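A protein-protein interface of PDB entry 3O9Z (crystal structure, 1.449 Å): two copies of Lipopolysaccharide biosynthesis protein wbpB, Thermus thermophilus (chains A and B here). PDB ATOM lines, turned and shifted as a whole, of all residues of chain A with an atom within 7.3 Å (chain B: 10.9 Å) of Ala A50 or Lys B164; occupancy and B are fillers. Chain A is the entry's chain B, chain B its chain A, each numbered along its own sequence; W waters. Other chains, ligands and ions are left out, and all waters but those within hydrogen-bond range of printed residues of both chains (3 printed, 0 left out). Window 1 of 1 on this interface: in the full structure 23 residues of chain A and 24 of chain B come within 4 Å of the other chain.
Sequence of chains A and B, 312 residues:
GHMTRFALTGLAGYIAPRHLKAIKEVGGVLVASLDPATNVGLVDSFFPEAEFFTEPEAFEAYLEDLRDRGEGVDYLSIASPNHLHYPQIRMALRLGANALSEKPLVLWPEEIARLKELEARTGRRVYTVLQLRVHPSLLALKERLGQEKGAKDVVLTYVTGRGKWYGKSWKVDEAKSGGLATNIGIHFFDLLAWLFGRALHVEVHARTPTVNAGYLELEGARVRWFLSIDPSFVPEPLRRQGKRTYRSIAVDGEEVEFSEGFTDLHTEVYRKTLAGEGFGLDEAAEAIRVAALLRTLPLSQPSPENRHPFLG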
ATOM      1  N   PHE A   6       2.021  -0.955 -27.125  1.00  0.00           N
ATOM      2  CA  PHE A   6       1.491   0.377 -27.503  1.00  0.00           C
ATOM      3  C   PHE A   6       0.699   1.042 -26.386  1.00  0.00           C
ATOM      4  O   PHE A   6       0.054   0.336 -25.601  1.00  0.00           O
ATOM      5  CB  PHE A   6       0.510   0.241 -28.680  1.00  0.00           C
ATOM      6  CG  PHE A   6       1.164  -0.105 -30.001  1.00  0.00           C
ATOM      7  CD1 PHE A   6       1.399  -1.423 -30.362  1.00  0.00           C
ATOM      8  CD2 PHE A   6       1.479   0.914 -30.888  1.00  0.00           C
ATOM      9  CE1 PHE A   6       1.997  -1.725 -31.613  1.00  0.00           C
ATOM     10  CE2 PHE A   6       2.127   0.617 -32.094  1.00  0.00           C
ATOM     11  CZ  PHE A   6       2.310  -0.677 -32.482  1.00  0.00           C
ATOM     12  N   LEU A  11      -8.550   7.591 -27.842  1.00  0.00           N
ATOM     13  CA  LEU A  11      -9.292   6.329 -27.953  1.00  0.00           C
ATOM     14  C   LEU A  11     -10.805   6.451 -28.278  1.00  0.00           C
ATOM     15  O   LEU A  11     -11.342   5.549 -28.934  1.00  0.00           O
ATOM     16  CB  LEU A  11      -9.132   5.543 -26.630  1.00  0.00           C
ATOM     17  CG  LEU A  11      -9.865   4.186 -26.573  1.00  0.00           C
ATOM     18  CD1 LEU A  11      -9.273   3.196 -27.536  1.00  0.00           C
ATOM     19  CD2 LEU A  11      -9.792   3.694 -25.141  1.00  0.00           C
ATOM     20  N   VAL A  29       0.169  -5.263 -28.557  1.00  0.00           N
ATOM     21  CA  VAL A  29      -0.754  -5.158 -27.414  1.00  0.00           C
ATOM     22  C   VAL A  29      -0.941  -3.703 -26.998  1.00  0.00           C
ATOM     23  O   VAL A  29       0.011  -2.938 -26.853  1.00  0.00           O
ATOM     24  CB  VAL A  29      -0.294  -5.992 -26.200  1.00  0.00           C
ATOM     25  CG1 VAL A  29       1.049  -5.524 -25.691  1.00  0.00           C
ATOM     26  CG2 VAL A  29      -1.366  -5.934 -25.072  1.00  0.00           C
ATOM     27  N   LEU A  30      -2.206  -3.337 -26.754  1.00  0.00           N
ATOM     28  CA  LEU A  30      -2.498  -2.003 -26.222  1.00  0.00           C
ATOM     29  C   LEU A  30      -2.420  -2.067 -24.710  1.00  0.00           C
ATOM     30  O   LEU A  30      -3.253  -2.730 -24.075  1.00  0.00           O
ATOM     31  CB  LEU A  30      -3.913  -1.562 -26.646  1.00  0.00           C
ATOM     32  CG  LEU A  30      -4.344  -0.214 -26.036  1.00  0.00           C
ATOM     33  CD1 LEU A  30      -3.501   0.908 -26.662  1.00  0.00           C
ATOM     34  CD2 LEU A  30      -5.832   0.004 -26.352  1.00  0.00           C
ATOM     35  N   VAL A  31      -1.456  -1.372 -24.139  1.00  0.00           N
ATOM     36  CA  VAL A  31      -1.194  -1.422 -22.710  1.00  0.00           C
ATOM     37  C   VAL A  31      -2.073  -0.410 -21.963  1.00  0.00           C
ATOM     38  O   VAL A  31      -2.563  -0.672 -20.858  1.00  0.00           O
ATOM     39  CB  VAL A  31       0.307  -1.154 -22.416  1.00  0.00           C
ATOM     40  CG1 VAL A  31       0.587  -1.129 -20.919  1.00  0.00           C
ATOM     41  CG2 VAL A  31       1.140  -2.245 -23.086  1.00  0.00           C
ATOM     42  N   ALA A  32      -2.286   0.753 -22.568  1.00  0.00           N
ATOM     43  CA  ALA A  32      -2.996   1.831 -21.893  1.00  0.00           C
ATOM     44  C   ALA A  32      -3.431   2.848 -22.925  1.00  0.00           C
ATOM     45  O   ALA A  32      -2.824   2.979 -24.008  1.00  0.00           O
ATOM     46  CB  ALA A  32      -2.121   2.535 -20.891  1.00  0.00           C
ATOM     47  N   SER A  33      -4.505   3.578 -22.590  1.00  0.00           N
ATOM     48  CA  SER A  33      -5.004   4.650 -23.448  1.00  0.00           C
ATOM     49  C   SER A  33      -5.355   5.891 -22.640  1.00  0.00           C
ATOM     50  O   SER A  33      -5.619   5.837 -21.412  1.00  0.00           O
ATOM     51  CB  SER A  33      -6.288   4.230 -24.200  1.00  0.00           C
ATOM     52  OG  SER A  33      -6.227   2.942 -24.785  1.00  0.00           O
ATOM     53  N   VAL A  40     -15.704   5.170 -24.817  1.00  0.00           N
ATOM     54  CA  VAL A  40     -14.688   4.288 -25.364  1.00  0.00           C
ATOM     55  C   VAL A  40     -14.942   2.812 -25.263  1.00  0.00           C
ATOM     56  O   VAL A  40     -14.027   1.992 -25.468  1.00  0.00           O
ATOM     57  CB  VAL A  40     -13.291   4.554 -24.669  1.00  0.00           C
ATOM     58  CG1 VAL A  40     -12.874   6.044 -24.761  1.00  0.00           C
ATOM     59  CG2 VAL A  40     -13.352   4.125 -23.177  1.00  0.00           C
ATOM     60  N   VAL A  43     -13.358  -0.421 -26.934  1.00  0.00           N
ATOM     61  CA  VAL A  43     -12.010  -0.924 -26.659  1.00  0.00           C
ATOM     62  C   VAL A  43     -12.032  -2.341 -26.098  1.00  0.00           C
ATOM     63  O   VAL A  43     -11.097  -3.107 -26.332  1.00  0.00           O
ATOM     64  CB  VAL A  43     -11.228   0.038 -25.750  1.00  0.00           C
ATOM     65  CG1 VAL A  43     -11.784   0.082 -24.313  1.00  0.00           C
ATOM     66  CG2 VAL A  43      -9.736  -0.331 -25.726  1.00  0.00           C
ATOM     67  N   ASP A  44     -13.066  -2.711 -25.340  1.00  0.00           N
ATOM     68  CA  ASP A  44     -13.032  -4.045 -24.737  1.00  0.00           C
ATOM     69  C   ASP A  44     -13.108  -5.177 -25.753  1.00  0.00           C
ATOM     70  O   ASP A  44     -12.657  -6.267 -25.439  1.00  0.00           O
ATOM     71  CB  ASP A  44     -14.207  -4.211 -23.770  1.00  0.00           C
ATOM     72  CG  ASP A  44     -13.971  -3.496 -22.449  1.00  0.00           C
ATOM     73  OD1 ASP A  44     -12.871  -2.972 -22.191  1.00  0.00           O
ATOM     74  OD2 ASP A  44     -14.897  -3.467 -21.615  1.00  0.00           O
ATOM     75  N   PHE A  47      -8.932  -5.008 -26.744  1.00  0.00           N
ATOM     76  CA  PHE A  47      -7.946  -5.111 -25.680  1.00  0.00           C
ATOM     77  C   PHE A  47      -8.612  -4.929 -24.311  1.00  0.00           C
ATOM     78  O   PHE A  47      -8.575  -3.871 -23.712  1.00  0.00           O
ATOM     79  CB  PHE A  47      -6.837  -4.077 -25.910  1.00  0.00           C
ATOM     80  CG  PHE A  47      -6.045  -4.357 -27.175  1.00  0.00           C
ATOM     81  CD1 PHE A  47      -5.184  -5.456 -27.243  1.00  0.00           C
ATOM     82  CD2 PHE A  47      -6.283  -3.615 -28.312  1.00  0.00           C
ATOM     83  CE1 PHE A  47      -4.478  -5.737 -28.437  1.00  0.00           C
ATOM     84  CE2 PHE A  47      -5.614  -3.907 -29.485  1.00  0.00           C
ATOM     85  CZ  PHE A  47      -4.718  -4.964 -29.553  1.00  0.00           C
ATOM     86  N   PRO A  48      -9.252  -5.995 -23.817  1.00  0.00           N
ATOM     87  CA  PRO A  48     -10.073  -5.887 -22.610  1.00  0.00           C
ATOM     88  C   PRO A  48      -9.288  -5.654 -21.328  1.00  0.00           C
ATOM     89  O   PRO A  48      -9.893  -5.320 -20.299  1.00  0.00           O
ATOM     90  CB  PRO A  48     -10.801  -7.233 -22.574  1.00  0.00           C
ATOM     91  CG  PRO A  48      -9.963  -8.177 -23.397  1.00  0.00           C
ATOM     92  CD  PRO A  48      -9.366  -7.306 -24.483  1.00  0.00           C
ATOM     93  N   GLU A  49      -7.954  -5.691 -21.357  1.00  0.00           N
ATOM     94  CA  GLU A  49      -7.161  -5.467 -20.145  1.00  0.00           C
ATOM     95  C   GLU A  49      -6.373  -4.155 -20.131  1.00  0.00           C
ATOM     96  O   GLU A  49      -5.660  -3.831 -19.173  1.00  0.00           O
ATOM     97  CB  GLU A  49      -6.203  -6.647 -19.865  1.00  0.00           C
ATOM     98  CG  GLU A  49      -7.051  -7.911 -19.649  1.00  0.00           C
ATOM     99  CD  GLU A  49      -6.270  -9.159 -19.304  1.00  0.00           C
ATOM    100  OE1 GLU A  49      -5.025  -9.124 -19.294  1.00  0.00           O
ATOM    101  OE2 GLU A  49      -6.928 -10.189 -19.042  1.00  0.00           O
ATOM    102  N   ALA A  50      -6.588  -3.313 -21.145  1.00  0.00           N
ATOM    103  CA  ALA A  50      -5.839  -2.078 -21.253  1.00  0.00           C
ATOM    104  C   ALA A  50      -6.199  -1.118 -20.127  1.00  0.00           C
ATOM    105  O   ALA A  50      -7.384  -1.015 -19.764  1.00  0.00           O
ATOM    106  CB  ALA A  50      -6.090  -1.402 -22.616  1.00  0.00           C
ATOM    107  N   GLU A  51      -5.239  -0.392 -19.545  1.00  0.00           N
ATOM    108  CA  GLU A  51      -5.468   0.662 -18.591  1.00  0.00           C
ATOM    109  C   GLU A  51      -6.068   1.850 -19.341  1.00  0.00           C
ATOM    110  O   GLU A  51      -5.942   1.974 -20.565  1.00  0.00           O
ATOM    111  CB  GLU A  51      -4.186   1.035 -17.851  1.00  0.00           C
ATOM    112  CG  GLU A  51      -3.502  -0.125 -17.144  1.00  0.00           C
ATOM    113  CD  GLU A  51      -4.198  -0.734 -15.951  1.00  0.00           C
ATOM    114  OE1 GLU A  51      -3.816  -1.882 -15.622  1.00  0.00           O
ATOM    115  OE2 GLU A  51      -5.068  -0.099 -15.320  1.00  0.00           O
ATOM    116  N   PHE A  52      -6.783   2.697 -18.595  1.00  0.00           N
ATOM    117  CA  PHE A  52      -7.447   3.851 -19.214  1.00  0.00           C
ATOM    118  C   PHE A  52      -7.334   5.036 -18.302  1.00  0.00           C
ATOM    119  O   PHE A  52      -7.511   4.934 -17.081  1.00  0.00           O
ATOM    120  CB  PHE A  52      -8.924   3.521 -19.536  1.00  0.00           C
ATOM    121  CG  PHE A  52      -9.628   4.699 -20.166  1.00  0.00           C
ATOM    122  CD1 PHE A  52      -9.408   5.053 -21.488  1.00  0.00           C
ATOM    123  CD2 PHE A  52     -10.397   5.540 -19.391  1.00  0.00           C
ATOM    124  CE1 PHE A  52     -10.009   6.169 -22.068  1.00  0.00           C
ATOM    125  CE2 PHE A  52     -11.028   6.682 -19.938  1.00  0.00           C
ATOM    126  CZ  PHE A  52     -10.784   7.016 -21.280  1.00  0.00           C
ATOM    127  N   PHE A  53      -7.094   6.199 -18.926  1.00  0.00           N
ATOM    128  CA  PHE A  53      -6.938   7.463 -18.214  1.00  0.00           C
ATOM    129  C   PHE A  53      -7.728   8.544 -18.930  1.00  0.00           C
ATOM    130  O   PHE A  53      -7.718   8.635 -20.151  1.00  0.00           O
ATOM    131  CB  PHE A  53      -5.436   7.862 -18.187  1.00  0.00           C
ATOM    132  CG  PHE A  53      -4.586   6.891 -17.410  1.00  0.00           C
ATOM    133  CD1 PHE A  53      -4.359   7.020 -16.054  1.00  0.00           C
ATOM    134  CD2 PHE A  53      -4.116   5.756 -18.057  1.00  0.00           C
ATOM    135  CE1 PHE A  53      -3.598   6.023 -15.365  1.00  0.00           C
ATOM    136  CE2 PHE A  53      -3.402   4.765 -17.352  1.00  0.00           C
ATOM    137  CZ  PHE A  53      -3.161   4.922 -16.018  1.00  0.00           C
ATOM    138  N   TYR A  62       1.775   7.071 -15.016  1.00  0.00           N
ATOM    139  CA  TYR A  62       1.682   5.643 -15.194  1.00  0.00           C
ATOM    140  C   TYR A  62       2.700   5.089 -16.200  1.00  0.00           C
ATOM    141  O   TYR A  62       3.351   4.065 -15.930  1.00  0.00           O
ATOM    142  CB  TYR A  62       0.233   5.268 -15.617  1.00  0.00           C
ATOM    143  CG  TYR A  62       0.084   3.814 -15.949  1.00  0.00           C
ATOM    144  CD1 TYR A  62       0.112   2.879 -14.915  1.00  0.00           C
ATOM    145  CD2 TYR A  62      -0.005   3.372 -17.256  1.00  0.00           C
ATOM    146  CE1 TYR A  62       0.025   1.524 -15.160  1.00  0.00           C
ATOM    147  CE2 TYR A  62      -0.099   1.988 -17.490  1.00  0.00           C
ATOM    148  CZ  TYR A  62      -0.098   1.103 -16.444  1.00  0.00           C
ATOM    149  OH  TYR A  62      -0.199  -0.265 -16.632  1.00  0.00           O
ATOM    150  N   THR B 160     -20.828  -9.662 -17.171  1.00  0.00           N
ATOM    151  CA  THR B 160     -20.475  -9.043 -18.440  1.00  0.00           C
ATOM    152  C   THR B 160     -19.252  -8.148 -18.224  1.00  0.00           C
ATOM    153  O   THR B 160     -19.323  -7.120 -17.537  1.00  0.00           O
ATOM    154  CB  THR B 160     -21.689  -8.328 -19.071  1.00  0.00           C
ATOM    155  OG1 THR B 160     -21.274  -7.763 -20.330  1.00  0.00           O
ATOM    156  CG2 THR B 160     -22.209  -7.218 -18.162  1.00  0.00           C
ATOM    157  N   GLY B 161     -18.079  -8.596 -18.681  1.00  0.00           N
ATOM    158  CA  GLY B 161     -16.849  -7.939 -18.248  1.00  0.00           C
ATOM    159  C   GLY B 161     -16.748  -6.516 -18.767  1.00  0.00           C
ATOM    160  O   GLY B 161     -17.177  -6.208 -19.881  1.00  0.00           O
ATOM    161  N   ARG B 162     -16.159  -5.679 -17.915  1.00  0.00           N
ATOM    162  CA  ARG B 162     -15.912  -4.277 -18.309  1.00  0.00           C
ATOM    163  C   ARG B 162     -14.476  -3.914 -17.988  1.00  0.00           C
ATOM    164  O   ARG B 162     -13.974  -4.121 -16.872  1.00  0.00           O
ATOM    165  CB  ARG B 162     -16.843  -3.301 -17.577  1.00  0.00           C
ATOM    166  CG  ARG B 162     -18.294  -3.439 -18.011  1.00  0.00           C
ATOM    167  CD  ARG B 162     -18.541  -2.913 -19.430  1.00  0.00           C
ATOM    168  NE  ARG B 162     -19.951  -2.985 -19.783  1.00  0.00           N
ATOM    169  CZ  ARG B 162     -20.559  -4.090 -20.188  1.00  0.00           C
ATOM    170  NH1 ARG B 162     -19.912  -5.247 -20.216  1.00  0.00           N
ATOM    171  NH2 ARG B 162     -21.863  -4.048 -20.512  1.00  0.00           N
ATOM    172  N   GLY B 163     -13.873  -3.258 -18.980  1.00  0.00           N
ATOM    173  CA  GLY B 163     -12.501  -2.786 -18.753  1.00  0.00           C
ATOM    174  C   GLY B 163     -12.361  -1.556 -17.876  1.00  0.00           C
ATOM    175  O   GLY B 163     -13.347  -1.016 -17.350  1.00  0.00           O
ATOM    176  N   LYS B 164     -11.125  -1.081 -17.736  1.00  0.00           N
ATOM    177  CA  LYS B 164     -10.770  -0.043 -16.770  1.00  0.00           C
ATOM    178  C   LYS B 164     -11.413   1.298 -17.072  1.00  0.00           C
ATOM    179  O   LYS B 164     -11.567   2.131 -16.180  1.00  0.00           O
ATOM    180  CB  LYS B 164      -9.238   0.098 -16.773  1.00  0.00           C
ATOM    181  CG  LYS B 164      -8.569  -1.099 -16.149  1.00  0.00           C
ATOM    182  CD  LYS B 164      -8.866  -1.255 -14.722  1.00  0.00           C
ATOM    183  CE  LYS B 164      -8.061  -2.459 -14.241  1.00  0.00           C
ATOM    184  NZ  LYS B 164      -7.342  -1.950 -13.066  1.00  0.00           N
ATOM    185  N   TRP B 165     -11.851   1.518 -18.303  1.00  0.00           N
ATOM    186  CA  TRP B 165     -12.505   2.773 -18.638  1.00  0.00           C
ATOM    187  C   TRP B 165     -13.837   2.909 -17.876  1.00  0.00           C
ATOM    188  O   TRP B 165     -14.269   4.021 -17.609  1.00  0.00           O
ATOM    189  CB  TRP B 165     -12.734   2.839 -20.164  1.00  0.00           C
ATOM    190  CG  TRP B 165     -13.536   1.681 -20.650  1.00  0.00           C
ATOM    191  CD1 TRP B 165     -13.051   0.451 -21.003  1.00  0.00           C
ATOM    192  CD2 TRP B 165     -14.967   1.579 -20.729  1.00  0.00           C
ATOM    193  NE1 TRP B 165     -14.080  -0.412 -21.327  1.00  0.00           N
ATOM    194  CE2 TRP B 165     -15.266   0.256 -21.147  1.00  0.00           C
ATOM    195  CE3 TRP B 165     -16.021   2.497 -20.495  1.00  0.00           C
ATOM    196  CZ2 TRP B 165     -16.588  -0.195 -21.345  1.00  0.00           C
ATOM    197  CZ3 TRP B 165     -17.338   2.052 -20.757  1.00  0.00           C
ATOM    198  CH2 TRP B 165     -17.574   0.720 -21.107  1.00  0.00           C
ATOM    199  N   TYR B 166     -14.528   1.798 -17.658  1.00  0.00           N
ATOM    200  CA  TYR B 166     -15.881   1.879 -17.055  1.00  0.00           C
ATOM    201  C   TYR B 166     -15.828   2.609 -15.719  1.00  0.00           C
ATOM    202  O   TYR B 166     -16.693   3.467 -15.445  1.00  0.00           O
ATOM    203  CB  TYR B 166     -16.422   0.443 -16.971  1.00  0.00           C
ATOM    204  CG  TYR B 166     -17.839   0.295 -16.504  1.00  0.00           C
ATOM    205  CD1 TYR B 166     -18.851   0.094 -17.426  1.00  0.00           C
ATOM    206  CD2 TYR B 166     -18.150   0.248 -15.149  1.00  0.00           C
ATOM    207  CE1 TYR B 166     -20.179  -0.092 -16.994  1.00  0.00           C
ATOM    208  CE2 TYR B 166     -19.482   0.055 -14.701  1.00  0.00           C
ATOM    209  CZ  TYR B 166     -20.441  -0.097 -15.633  1.00  0.00           C
ATOM    210  OH  TYR B 166     -21.780  -0.298 -15.244  1.00  0.00           O
ATOM    211  N   GLY B 167     -14.832   2.313 -14.877  1.00  0.00           N
ATOM    212  CA  GLY B 167     -14.665   2.973 -13.583  1.00  0.00           C
ATOM    213  C   GLY B 167     -14.291   4.434 -13.575  1.00  0.00           C
ATOM    214  O   GLY B 167     -14.260   5.051 -12.505  1.00  0.00           O
ATOM    215  N   LYS B 168     -14.023   4.983 -14.763  1.00  0.00           N
ATOM    216  CA  LYS B 168     -13.704   6.397 -14.940  1.00  0.00           C
ATOM    217  C   LYS B 168     -14.803   7.114 -15.708  1.00  0.00           C
ATOM    218  O   LYS B 168     -14.663   8.297 -16.024  1.00  0.00           O
ATOM    219  CB  LYS B 168     -12.334   6.573 -15.616  1.00  0.00           C
ATOM    220  CG  LYS B 168     -11.269   6.063 -14.641  1.00  0.00           C
ATOM    221  CD  LYS B 168      -9.868   6.439 -15.151  1.00  0.00           C
ATOM    222  CE  LYS B 168      -8.871   5.966 -14.102  1.00  0.00           C
ATOM    223  NZ  LYS B 168      -7.434   6.176 -14.585  1.00  0.00           N
ATOM    224  N   SER B 169     -15.934   6.428 -15.889  1.00  0.00           N
ATOM    225  CA  SER B 169     -17.052   6.986 -16.690  1.00  0.00           C
ATOM    226  C   SER B 169     -18.257   7.304 -15.795  1.00  0.00           C
ATOM    227  O   SER B 169     -18.323   6.950 -14.609  1.00  0.00           O
ATOM    228  CB  SER B 169     -17.423   5.951 -17.753  1.00  0.00           C
ATOM    229  OG  SER B 169     -18.232   4.931 -17.203  1.00  0.00           O
ATOM    230  N   TRP B 170     -19.254   7.927 -16.436  1.00  0.00           N
ATOM    231  CA  TRP B 170     -20.522   8.210 -15.760  1.00  0.00           C
ATOM    232  C   TRP B 170     -21.177   6.931 -15.270  1.00  0.00           C
ATOM    233  O   TRP B 170     -22.054   6.979 -14.408  1.00  0.00           O
ATOM    234  CB  TRP B 170     -21.470   8.952 -16.711  1.00  0.00           C
ATOM    235  CG  TRP B 170     -21.882   8.139 -17.915  1.00  0.00           C
ATOM    236  CD1 TRP B 170     -21.315   8.156 -19.167  1.00  0.00           C
ATOM    237  CD2 TRP B 170     -22.985   7.235 -18.015  1.00  0.00           C
ATOM    238  NE1 TRP B 170     -21.938   7.287 -19.999  1.00  0.00           N
ATOM    239  CE2 TRP B 170     -22.981   6.697 -19.318  1.00  0.00           C
ATOM    240  CE3 TRP B 170     -23.958   6.776 -17.096  1.00  0.00           C
ATOM    241  CZ2 TRP B 170     -23.915   5.761 -19.744  1.00  0.00           C
ATOM    242  CZ3 TRP B 170     -24.872   5.826 -17.523  1.00  0.00           C
ATOM    243  CH2 TRP B 170     -24.827   5.287 -18.814  1.00  0.00           C
ATOM    244  N   LYS B 171     -20.838   5.788 -15.857  1.00  0.00           N
ATOM    245  CA  LYS B 171     -21.453   4.520 -15.483  1.00  0.00           C
ATOM    246  C   LYS B 171     -21.332   4.143 -14.038  1.00  0.00           C
ATOM    247  O   LYS B 171     -22.168   3.394 -13.498  1.00  0.00           O
ATOM    248  CB  LYS B 171     -21.046   3.396 -16.462  1.00  0.00           C
ATOM    249  CG  LYS B 171     -21.533   3.685 -17.906  1.00  0.00           C
ATOM    250  CD  LYS B 171     -20.607   3.053 -18.946  1.00  0.00           C
ATOM    251  CE  LYS B 171     -21.032   3.371 -20.368  1.00  0.00           C
ATOM    252  NZ  LYS B 171     -22.090   2.403 -20.841  1.00  0.00           N
ATOM    253  N   VAL B 172     -20.273   4.598 -13.378  1.00  0.00           N
ATOM    254  CA  VAL B 172     -20.128   4.307 -11.960  1.00  0.00           C
ATOM    255  C   VAL B 172     -20.508   5.484 -11.056  1.00  0.00           C
ATOM    256  O   VAL B 172     -20.382   5.382  -9.826  1.00  0.00           O
ATOM    257  CB  VAL B 172     -18.692   3.823 -11.593  1.00  0.00           C
ATOM    258  CG1 VAL B 172     -18.362   2.560 -12.411  1.00  0.00           C
ATOM    259  CG2 VAL B 172     -17.688   4.975 -11.885  1.00  0.00           C
ATOM    260  N   THR B 210     -18.020  -4.085  -8.224  1.00  0.00           N
ATOM    261  CA  THR B 210     -18.127  -4.926  -9.398  1.00  0.00           C
ATOM    262  C   THR B 210     -19.077  -6.107  -9.207  1.00  0.00           C
ATOM    263  O   THR B 210     -19.278  -6.830 -10.179  1.00  0.00           O
ATOM    264  CB  THR B 210     -16.774  -5.501  -9.793  1.00  0.00           C
ATOM    265  OG1 THR B 210     -16.249  -6.148  -8.629  1.00  0.00           O
ATOM    266  CG2 THR B 210     -15.837  -4.333 -10.209  1.00  0.00           C
ATOM    267  N   ILE B 229     -19.510  -7.242 -13.221  1.00  0.00           N
ATOM    268  CA  ILE B 229     -18.733  -6.747 -14.357  1.00  0.00           C
ATOM    269  C   ILE B 229     -17.279  -7.184 -14.286  1.00  0.00           C
ATOM    270  O   ILE B 229     -16.445  -6.691 -15.063  1.00  0.00           O
ATOM    271  CB  ILE B 229     -18.869  -5.214 -14.566  1.00  0.00           C
ATOM    272  CG1 ILE B 229     -18.523  -4.528 -13.253  1.00  0.00           C
ATOM    273  CG2 ILE B 229     -20.304  -4.886 -15.040  1.00  0.00           C
ATOM    274  CD1 ILE B 229     -18.335  -2.978 -13.336  1.00  0.00           C
ATOM    275  N   ASP B 230     -16.983  -8.068 -13.333  1.00  0.00           N
ATOM    276  CA  ASP B 230     -15.642  -8.711 -13.266  1.00  0.00           C
ATOM    277  C   ASP B 230     -15.716 -10.050 -14.010  1.00  0.00           C
ATOM    278  O   ASP B 230     -16.398 -10.970 -13.547  1.00  0.00           O
ATOM    279  CB  ASP B 230     -15.291  -8.905 -11.796  1.00  0.00           C
ATOM    280  CG  ASP B 230     -13.940  -9.535 -11.581  1.00  0.00           C
ATOM    281  OD1 ASP B 230     -13.368 -10.032 -12.570  1.00  0.00           O
ATOM    282  OD2 ASP B 230     -13.508  -9.563 -10.403  1.00  0.00           O
ATOM    283  N   PRO B 231     -15.000 -10.165 -15.136  1.00  0.00           N
ATOM    284  CA  PRO B 231     -15.116 -11.396 -15.924  1.00  0.00           C
ATOM    285  C   PRO B 231     -14.458 -12.621 -15.264  1.00  0.00           C
ATOM    286  O   PRO B 231     -14.710 -13.734 -15.711  1.00  0.00           O
ATOM    287  CB  PRO B 231     -14.400 -11.013 -17.227  1.00  0.00           C
ATOM    288  CG  PRO B 231     -13.341 -10.061 -16.790  1.00  0.00           C
ATOM    289  CD  PRO B 231     -14.090  -9.183 -15.760  1.00  0.00           C
ATOM    290  N   ARG B 244     -15.707 -13.597 -21.765  1.00  0.00           N
ATOM    291  CA  ARG B 244     -15.846 -12.553 -20.741  1.00  0.00           C
ATOM    292  C   ARG B 244     -17.285 -12.206 -20.399  1.00  0.00           C
ATOM    293  O   ARG B 244     -17.523 -11.247 -19.660  1.00  0.00           O
ATOM    294  CB  ARG B 244     -15.058 -11.304 -21.140  1.00  0.00           C
ATOM    295  CG  ARG B 244     -13.590 -11.647 -21.306  1.00  0.00           C
ATOM    296  CD  ARG B 244     -12.714 -10.494 -21.754  1.00  0.00           C
ATOM    297  NE  ARG B 244     -11.357 -10.870 -21.380  1.00  0.00           N
ATOM    298  CZ  ARG B 244     -10.715 -10.391 -20.321  1.00  0.00           C
ATOM    299  NH1 ARG B 244     -11.253  -9.439 -19.572  1.00  0.00           N
ATOM    300  NH2 ARG B 244      -9.497 -10.833 -20.058  1.00  0.00           N
HETATM  301  O   HOH W   1      -9.237  -2.811 -19.081  1.00  0.00           O
HETATM  302  O   HOH W   2     -17.319  -4.158 -22.393  1.00  0.00           O
HETATM  303  O   HOH W   3     -12.158  -6.332 -19.048  1.00  0.00           O
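Ala A50 touches one residue of chain B.
No residue of chain B comes within 4 Å of Leu A30.
No residue of chain B comes within 4 Å of Ala A32.
Glu A51 touches just one residue of chain B: Lys B164 (3.7 Å).
Of the printed residues of chain A, Trp B165 touches Val A40 (3.3 Å), Val A43 (3.6 Å), Asp A44 (3.0 Å) and Phe A52 (3.6 Å).
Of the printed residues of chain A, Arg B244 touches Pro A48 (3.6 Å) and Glu A49 (2.8 Å).
Of the printed residues of chain A, Gly B161 touches Asp A44 (3.96 Å).
Lys B171 touches none of the printed residues of chain A.
The nearest printed residue of chain B that does not touch Ala A50 is Trp B165 (5.3 Å).
The nearest printed residue of chain A that does not touch Lys B164 is Phe A52 (4.01 Å).
The nearest printed residue of chain A that does not touch Arg B244 is Asp A44 (5.6 Å).
Water W2 bridges OD2 of Asp A44 (2.6 Å) and O of Gly B161 (3.2 Å).
Water W1 lies within hydrogen-bond range of O of Ala A50 (2.7 Å), O of Pro A48 (2.9 Å) and N of Lys B164 (2.9 Å).
Water W3 lies within hydrogen-bond range of O of Pro A48 (2.8 Å) and NH1 of Arg B244 (3.3 Å).
Of the 18 printed residues of chain A, 9 touch a printed residue of chain B.
Printed residues of chain A that touch a printed residue of chain B: Val A40, Val A43, Asp A44, Pro A48, Glu A49, Ala A50, Glu A51, Phe A52 and Phe A53.
Of the 18 printed residues of chain B, 7 touch a printed residue of chain A.
Hydrophobic or aromatic side chains of chain B that line the printed part of chain A: Trp B165.
Among the printed residues, Asp or Glu carboxylates within 4 Å of a Lys or Arg side-chain nitrogen of the other chain: Glu A49 with Arg B244 (2.8 Å) and Glu A51 with Lys B164 (3.7 Å).
The side-chain hydroxyl (OG1) of Thr B160 is in hydrogen-bond range of the guanidinium group (NH1) of Arg B162 (2.9 Å).
The backbone carbonyl oxygen (O) of Ile B229 sits at hydrogen-bond distance from the backbone NH (N) of Arg B162.
N of Ser A33 lies within hydrogen-bond range of O of Glu A51.
The side-chain carboxylate of Asp A44 sits at hydrogen-bond distance from the backbone NH of Gly B163 (2.8 Å).
NZ of Lys B164 is in salt-bridge range of OE2 of Glu A51.
The side-chain carboxylate of Asp A44 is in hydrogen-bond range of the indole nitrogen of Trp B165.
The side-chain amino group (NZ) of Lys B168 sits at hydrogen-bond distance from the backbone carbonyl oxygen (O) of Phe A52 (2.8 Å).
The guanidinium group (NH2) of Arg B244 lies within salt-bridge range of the side-chain carboxylate (OE2) of Glu A49, 2.8 Å away.
No position is printed for both chains.
Val A40 touches Trp B165 (CG2 to CB, 3.3 Å).
CG1 of Val A43 touches CD1 of Trp B165 (3.6 Å).
CA of Gly B163 touches O of Pro A48, at 3.95 Å.
CG of Pro A48 touches NE of Arg B244 (3.6 Å).
Ala A50 touches Lys B164.
Phe A52 touches Trp B165 (CD2 to CA, 3.6 Å).
Lys B168 touches Phe A53 (NZ to CD1, 3.5 Å).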
